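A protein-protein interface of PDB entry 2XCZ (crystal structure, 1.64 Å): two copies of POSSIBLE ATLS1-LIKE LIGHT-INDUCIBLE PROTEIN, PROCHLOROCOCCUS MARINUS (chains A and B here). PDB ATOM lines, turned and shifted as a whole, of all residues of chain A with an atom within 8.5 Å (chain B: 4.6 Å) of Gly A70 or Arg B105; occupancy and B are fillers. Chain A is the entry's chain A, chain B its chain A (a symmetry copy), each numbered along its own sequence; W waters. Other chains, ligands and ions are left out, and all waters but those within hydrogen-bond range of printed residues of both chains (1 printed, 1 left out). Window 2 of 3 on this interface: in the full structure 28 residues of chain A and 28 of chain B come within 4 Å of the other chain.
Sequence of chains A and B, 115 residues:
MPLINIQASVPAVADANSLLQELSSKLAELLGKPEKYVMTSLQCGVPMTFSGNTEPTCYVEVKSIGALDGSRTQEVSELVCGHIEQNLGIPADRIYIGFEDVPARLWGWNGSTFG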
ATOM      1  N   ALA A  67     -26.752 -17.715 -32.498  1.00  0.00           N
ATOM      2  CA  ALA A  67     -27.068 -18.697 -31.454  1.00  0.00           C
ATOM      3  C   ALA A  67     -25.829 -19.290 -30.778  1.00  0.00           C
ATOM      4  O   ALA A  67     -25.926 -20.297 -30.074  1.00  0.00           O
ATOM      5  CB  ALA A  67     -27.986 -19.797 -31.986  1.00  0.00           C
ATOM      6  N   LEU A  68     -24.681 -18.655 -30.992  1.00  0.00           N
ATOM      7  CA  LEU A  68     -23.423 -19.129 -30.423  1.00  0.00           C
ATOM      8  C   LEU A  68     -22.798 -18.069 -29.516  1.00  0.00           C
ATOM      9  O   LEU A  68     -21.579 -17.954 -29.420  1.00  0.00           O
ATOM     10  CB  LEU A  68     -22.447 -19.561 -31.547  1.00  0.00           C
ATOM     11  CG  LEU A  68     -22.929 -20.736 -32.415  1.00  0.00           C
ATOM     12  CD1 LEU A  68     -21.987 -20.958 -33.582  1.00  0.00           C
ATOM     13  CD2 LEU A  68     -23.052 -22.014 -31.574  1.00  0.00           C
ATOM     14  N   ASP A  69     -23.653 -17.315 -28.832  1.00  0.00           N
ATOM     15  CA  ASP A  69     -23.208 -16.245 -27.949  1.00  0.00           C
ATOM     16  C   ASP A  69     -22.964 -16.726 -26.515  1.00  0.00           C
ATOM     17  O   ASP A  69     -23.550 -17.723 -26.061  1.00  0.00           O
ATOM     18  CB  ASP A  69     -24.247 -15.117 -27.950  1.00  0.00           C
ATOM     19  CG  ASP A  69     -24.645 -14.683 -29.367  1.00  0.00           C
ATOM     20  OD1 ASP A  69     -23.762 -14.272 -30.145  1.00  0.00           O
ATOM     21  OD2 ASP A  69     -25.856 -14.712 -29.686  1.00  0.00           O
ATOM     22  N   GLY A  70     -22.100 -15.994 -25.813  1.00  0.00           N
ATOM     23  CA  GLY A  70     -21.823 -16.236 -24.400  1.00  0.00           C
ATOM     24  C   GLY A  70     -21.351 -17.653 -24.172  1.00  0.00           C
ATOM     25  O   GLY A  70     -20.386 -18.094 -24.792  1.00  0.00           O
ATOM     26  N   SER A  71     -22.071 -18.372 -23.320  1.00  0.00           N
ATOM     27  CA  SER A  71     -21.679 -19.725 -22.908  1.00  0.00           C
ATOM     28  C   SER A  71     -22.048 -20.820 -23.911  1.00  0.00           C
ATOM     29  O   SER A  71     -21.742 -21.995 -23.698  1.00  0.00           O
ATOM     30  CB  SER A  71     -22.298 -20.050 -21.548  1.00  0.00           C
ATOM     31  OG  SER A  71     -23.712 -20.048 -21.629  1.00  0.00           O
ATOM     32  N   ARG A  72     -22.694 -20.439 -25.009  1.00  0.00           N
ATOM     33  CA  ARG A  72     -23.223 -21.414 -25.955  1.00  0.00           C
ATOM     34  C   ARG A  72     -22.195 -22.381 -26.548  1.00  0.00           C
ATOM     35  O   ARG A  72     -22.473 -23.582 -26.639  1.00  0.00           O
ATOM     36  CB  ARG A  72     -24.000 -20.710 -27.072  1.00  0.00           C
ATOM     37  CG  ARG A  72     -25.424 -20.353 -26.698  1.00  0.00           C
ATOM     38  CD  ARG A  72     -26.338 -21.537 -26.949  1.00  0.00           C
ATOM     39  NE  ARG A  72     -27.710 -21.253 -26.532  1.00  0.00           N
ATOM     40  CZ  ARG A  72     -28.641 -20.691 -27.297  1.00  0.00           C
ATOM     41  NH1 ARG A  72     -28.379 -20.346 -28.554  1.00  0.00           N
ATOM     42  NH2 ARG A  72     -29.850 -20.481 -26.803  1.00  0.00           N
ATOM     43  N   THR A  73     -21.021 -21.879 -26.940  1.00  0.00           N
ATOM     44  CA  THR A  73     -20.020 -22.790 -27.521  1.00  0.00           C
ATOM     45  C   THR A  73     -19.528 -23.786 -26.475  1.00  0.00           C
ATOM     46  O   THR A  73     -19.319 -24.952 -26.802  1.00  0.00           O
ATOM     47  CB  THR A  73     -18.828 -22.082 -28.235  1.00  0.00           C
ATOM     48  OG1 THR A  73     -18.118 -21.267 -27.296  1.00  0.00           O
ATOM     49  CG2 THR A  73     -19.310 -21.235 -29.413  1.00  0.00           C
ATOM     50  N   GLN A  74     -19.393 -23.358 -25.213  1.00  0.00           N
ATOM     51  CA  GLN A  74     -19.104 -24.317 -24.129  1.00  0.00           C
ATOM     52  C   GLN A  74     -20.214 -25.368 -23.956  1.00  0.00           C
ATOM     53  O   GLN A  74     -19.938 -26.569 -23.840  1.00  0.00           O
ATOM     54  CB  GLN A  74     -18.800 -23.612 -22.790  1.00  0.00           C
ATOM     55  CG  GLN A  74     -17.348 -23.150 -22.655  1.00  0.00           C
ATOM     56  CD  GLN A  74     -16.993 -22.545 -21.283  1.00  0.00           C
ATOM     57  OE1 GLN A  74     -17.789 -22.569 -20.337  1.00  0.00           O
ATOM     58  NE2 GLN A  74     -15.780 -21.996 -21.185  1.00  0.00           N
ATOM     59  N   GLU A  75     -21.465 -24.915 -23.939  1.00  0.00           N
ATOM     60  CA  GLU A  75     -22.598 -25.802 -23.766  1.00  0.00           C
ATOM     61  C   GLU A  75     -22.755 -26.772 -24.927  1.00  0.00           C
ATOM     62  O   GLU A  75     -23.095 -27.936 -24.718  1.00  0.00           O
ATOM     63  CB  GLU A  75     -23.892 -24.991 -23.583  1.00  0.00           C
ATOM     64  CG  GLU A  75     -23.910 -24.187 -22.287  1.00  0.00           C
ATOM     65  CD  GLU A  75     -25.002 -23.134 -22.250  1.00  0.00           C
ATOM     66  OE1 GLU A  75     -25.871 -23.126 -23.146  1.00  0.00           O
ATOM     67  OE2 GLU A  75     -24.993 -22.305 -21.313  1.00  0.00           O
ATOM     68  N   SER A  77     -20.276 -27.768 -26.846  1.00  0.00           N
ATOM     69  CA  SER A  77     -19.163 -28.699 -26.726  1.00  0.00           C
ATOM     70  C   SER A  77     -19.469 -29.781 -25.681  1.00  0.00           C
ATOM     71  O   SER A  77     -19.197 -30.956 -25.900  1.00  0.00           O
ATOM     72  CB  SER A  77     -17.871 -27.957 -26.389  1.00  0.00           C
ATOM     73  OG  SER A  77     -16.808 -28.874 -26.258  1.00  0.00           O
ATOM     74  N   ILE A  97     -13.771 -29.533 -31.780  1.00  0.00           N
ATOM     75  CA  ILE A  97     -14.910 -28.936 -32.458  1.00  0.00           C
ATOM     76  C   ILE A  97     -14.534 -27.575 -33.002  1.00  0.00           C
ATOM     77  O   ILE A  97     -14.111 -26.682 -32.231  1.00  0.00           O
ATOM     78  CB  ILE A  97     -16.155 -28.799 -31.533  1.00  0.00           C
ATOM     79  CG1 ILE A  97     -16.517 -30.148 -30.880  1.00  0.00           C
ATOM     80  CG2 ILE A  97     -17.340 -28.259 -32.327  1.00  0.00           C
ATOM     81  CD1 ILE A  97     -17.517 -29.999 -29.735  1.00  0.00           C
ATOM     82  N   GLY A  98     -14.711 -27.388 -34.312  1.00  0.00           N
ATOM     83  CA  GLY A  98     -14.544 -26.046 -34.909  1.00  0.00           C
ATOM     84  C   GLY A  98     -15.901 -25.387 -35.073  1.00  0.00           C
ATOM     85  O   GLY A  98     -16.771 -25.914 -35.790  1.00  0.00           O
ATOM     86  N   PHE A  99     -16.078 -24.227 -34.432  1.00  0.00           N
ATOM     87  CA  PHE A  99     -17.341 -23.471 -34.506  1.00  0.00           C
ATOM     88  C   PHE A  99     -17.249 -22.300 -35.484  1.00  0.00           C
ATOM     89  O   PHE A  99     -16.198 -21.662 -35.592  1.00  0.00           O
ATOM     90  CB  PHE A  99     -17.685 -22.861 -33.131  1.00  0.00           C
ATOM     91  CG  PHE A  99     -18.116 -23.860 -32.099  1.00  0.00           C
ATOM     92  CD1 PHE A  99     -19.468 -24.190 -31.948  1.00  0.00           C
ATOM     93  CD2 PHE A  99     -17.180 -24.457 -31.261  1.00  0.00           C
ATOM     94  CE1 PHE A  99     -19.868 -25.087 -30.988  1.00  0.00           C
ATOM     95  CE2 PHE A  99     -17.563 -25.367 -30.279  1.00  0.00           C
ATOM     96  CZ  PHE A  99     -18.914 -25.703 -30.142  1.00  0.00           C
ATOM     97  N   GLU A 100     -18.364 -21.980 -36.142  1.00  0.00           N
ATOM     98  CA  GLU A 100     -18.460 -20.769 -36.958  1.00  0.00           C
ATOM     99  C   GLU A 100     -19.870 -20.183 -36.811  1.00  0.00           C
ATOM    100  O   GLU A 100     -20.864 -20.900 -36.929  1.00  0.00           O
ATOM    101  CB  GLU A 100     -18.172 -21.094 -38.426  1.00  0.00           C
ATOM    102  CG  GLU A 100     -18.179 -19.885 -39.358  1.00  0.00           C
ATOM    103  CD  GLU A 100     -17.682 -20.232 -40.753  1.00  0.00           C
ATOM    104  OE1 GLU A 100     -18.337 -21.036 -41.455  1.00  0.00           O
ATOM    105  OE2 GLU A 100     -16.619 -19.706 -41.149  1.00  0.00           O
ATOM    106  N   ASP A 101     -19.938 -18.892 -36.484  1.00  0.00           N
ATOM    107  CA  ASP A 101     -21.183 -18.138 -36.544  1.00  0.00           C
ATOM    108  C   ASP A 101     -21.220 -17.522 -37.945  1.00  0.00           C
ATOM    109  O   ASP A 101     -20.443 -16.610 -38.273  1.00  0.00           O
ATOM    110  CB  ASP A 101     -21.204 -17.076 -35.427  1.00  0.00           C
ATOM    111  CG  ASP A 101     -22.433 -16.174 -35.477  1.00  0.00           C
ATOM    112  OD1 ASP A 101     -23.219 -16.236 -36.453  1.00  0.00           O
ATOM    113  OD2 ASP A 101     -22.601 -15.376 -34.530  1.00  0.00           O
ATOM    114  N   PRO B 103     -10.668 -18.224 -33.128  1.00  0.00           N
ATOM    115  CA  PRO B 103     -10.641 -17.766 -31.740  1.00  0.00           C
ATOM    116  C   PRO B 103     -10.810 -18.941 -30.796  1.00  0.00           C
ATOM    117  O   PRO B 103     -11.558 -19.886 -31.100  1.00  0.00           O
ATOM    118  CB  PRO B 103     -11.847 -16.816 -31.659  1.00  0.00           C
ATOM    119  CG  PRO B 103     -12.054 -16.369 -33.057  1.00  0.00           C
ATOM    120  CD  PRO B 103     -11.766 -17.594 -33.876  1.00  0.00           C
ATOM    121  N   ALA B 104     -10.096 -18.906 -29.668  1.00  0.00           N
ATOM    122  CA  ALA B 104     -10.105 -20.012 -28.713  1.00  0.00           C
ATOM    123  C   ALA B 104     -11.518 -20.395 -28.252  1.00  0.00           C
ATOM    124  O   ALA B 104     -11.836 -21.584 -28.113  1.00  0.00           O
ATOM    125  CB  ALA B 104      -9.199 -19.699 -27.530  1.00  0.00           C
ATOM    126  N   ARG B 105     -12.382 -19.407 -28.051  1.00  0.00           N
ATOM    127  CA  ARG B 105     -13.768 -19.695 -27.637  1.00  0.00           C
ATOM    128  C   ARG B 105     -14.616 -20.395 -28.713  1.00  0.00           C
ATOM    129  O   ARG B 105     -15.702 -20.919 -28.409  1.00  0.00           O
ATOM    130  CB  ARG B 105     -14.471 -18.429 -27.144  1.00  0.00           C
ATOM    131  CG  ARG B 105     -14.677 -17.341 -28.176  1.00  0.00           C
ATOM    132  CD  ARG B 105     -15.571 -16.229 -27.600  1.00  0.00           C
ATOM    133  NE  ARG B 105     -16.926 -16.712 -27.287  1.00  0.00           N
ATOM    134  CZ  ARG B 105     -17.926 -16.774 -28.166  1.00  0.00           C
ATOM    135  NH1 ARG B 105     -17.749 -16.380 -29.422  1.00  0.00           N
ATOM    136  NH2 ARG B 105     -19.111 -17.223 -27.782  1.00  0.00           N
ATOM    137  N   LEU B 106     -14.106 -20.431 -29.944  1.00  0.00           N
ATOM    138  CA  LEU B 106     -14.751 -21.153 -31.056  1.00  0.00           C
ATOM    139  C   LEU B 106     -14.091 -22.510 -31.336  1.00  0.00           C
ATOM    140  O   LEU B 106     -14.324 -23.122 -32.383  1.00  0.00           O
ATOM    141  CB  LEU B 106     -14.782 -20.299 -32.333  1.00  0.00           C
ATOM    142  CG  LEU B 106     -15.546 -18.968 -32.234  1.00  0.00           C
ATOM    143  CD1 LEU B 106     -15.565 -18.231 -33.554  1.00  0.00           C
ATOM    144  CD2 LEU B 106     -16.955 -19.217 -31.711  1.00  0.00           C
ATOM    145  N   TRP B 107     -13.281 -22.977 -30.386  1.00  0.00           N
ATOM    146  CA  TRP B 107     -12.574 -24.231 -30.525  1.00  0.00           C
ATOM    147  C   TRP B 107     -12.927 -25.128 -29.339  1.00  0.00           C
ATOM    148  O   TRP B 107     -12.437 -24.928 -28.223  1.00  0.00           O
ATOM    149  CB  TRP B 107     -11.055 -23.997 -30.603  1.00  0.00           C
ATOM    150  CG  TRP B 107     -10.291 -25.202 -31.131  1.00  0.00           C
ATOM    151  CD1 TRP B 107     -10.334 -26.488 -30.652  1.00  0.00           C
ATOM    152  CD2 TRP B 107      -9.416 -25.224 -32.259  1.00  0.00           C
ATOM    153  NE1 TRP B 107      -9.530 -27.304 -31.415  1.00  0.00           N
ATOM    154  CE2 TRP B 107      -8.953 -26.554 -32.406  1.00  0.00           C
ATOM    155  CE3 TRP B 107      -8.988 -24.255 -33.171  1.00  0.00           C
ATOM    156  CZ2 TRP B 107      -8.059 -26.934 -33.414  1.00  0.00           C
ATOM    157  CZ3 TRP B 107      -8.095 -24.624 -34.176  1.00  0.00           C
ATOM    158  CH2 TRP B 107      -7.647 -25.964 -34.292  1.00  0.00           C
ATOM    159  N   THR B 113     -14.358 -25.353 -24.167  1.00  0.00           N
ATOM    160  CA  THR B 113     -13.592 -24.707 -25.251  1.00  0.00           C
ATOM    161  C   THR B 113     -12.260 -24.213 -24.704  1.00  0.00           C
ATOM    162  O   THR B 113     -12.060 -24.193 -23.489  1.00  0.00           O
ATOM    163  CB  THR B 113     -14.308 -23.474 -25.836  1.00  0.00           C
ATOM    164  OG1 THR B 113     -14.325 -22.429 -24.853  1.00  0.00           O
ATOM    165  CG2 THR B 113     -15.753 -23.781 -26.254  1.00  0.00           C
ATOM    166  N   GLY B 115     -11.330 -21.182 -24.760  1.00  0.00           N
ATOM    167  CA  GLY B 115     -11.521 -19.785 -24.333  1.00  0.00           C
ATOM    168  C   GLY B 115     -11.931 -19.645 -22.873  1.00  0.00           C
ATOM    169  O   GLY B 115     -11.713 -20.560 -22.064  1.00  0.00           O
HETATM  170  O   HOH W   1     -20.095 -15.853 -30.850  1.00  0.00           O
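Water W1 lies within hydrogen-bond range of the guanidinium group (NH1) of Arg B105 and the backbone carbonyl oxygen (O) of Leu A68.
No position is printed for both chains. Of the 10 pairs that touch across the chains among the printed residues, none has its exchanged pair printed and touching as well.
Of the printed residues of chain B, Leu A68 touches Arg B105. Of chain B, only Arg B105 (3.4 Å) comes within 4 Å of Gly A70. Printed residues of chain B within 4 Å of Thr A73: Arg B105, Leu B106 and Thr B113. Of the printed residues of chain B, Gly A98 touches Leu B106. Arg B105 touches three residues of chain A. Of the printed residues of chain A, Leu B106 touches Thr A73 (3.9 Å), Ile A97 (3.6 Å), Gly A98 (3.9 Å) and Phe A99 (2.9 Å). The nearest residue of chain A that does not touch Arg B105 is Asp A69 (4.1 Å). The nearest printed residue of chain A that does not touch Leu B106 is Glu A100 (5.1 Å).
Among the printed residues, pairs that only touch across the chains: Ile A97 with Trp B107 (3.4 Å), Ile A97 with Leu B106 (3.6 Å), Thr A73 with Thr B113 (3.6 Å), Gln A74 with Thr B113 (3.8 Å), Gly A98 with Leu B106 (3.9 Å) and Thr A73 with Leu B106 (3.9 Å).
O of Leu A68 sits at hydrogen-bond distance from NH2 of Arg B105 (3.1 Å). The backbone carbonyl oxygen (O) of Gly A70 sits at hydrogen-bond distance from the guanidinium group (NH2) of Arg B105, 3.4 Å away. OG1 of Thr A73 is in hydrogen-bond range of O of Arg B105, 2.7 Å away. The backbone NH (N) of Phe A99 lies within hydrogen-bond range of the backbone carbonyl oxygen (O) of Leu B106 (2.9 Å).
Of the 15 printed residues of chain A, 7 touch a printed residue of chain B. Printed residues of chain A that touch a printed residue of chain B: Leu A68, Gly A70, Thr A73, Gln A74, Ile A97, Gly A98 and Phe A99. Of the 7 printed residues of chain B, 4 touch a printed residue of chain A. Hydrophobic or aromatic side chains of chain B that line the printed part of chain A: Leu B106.
The side-chain hydroxyl (OG1) of Thr B113 lies close to the backbone NH (N) of Gly B115, at 3.2 Å.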
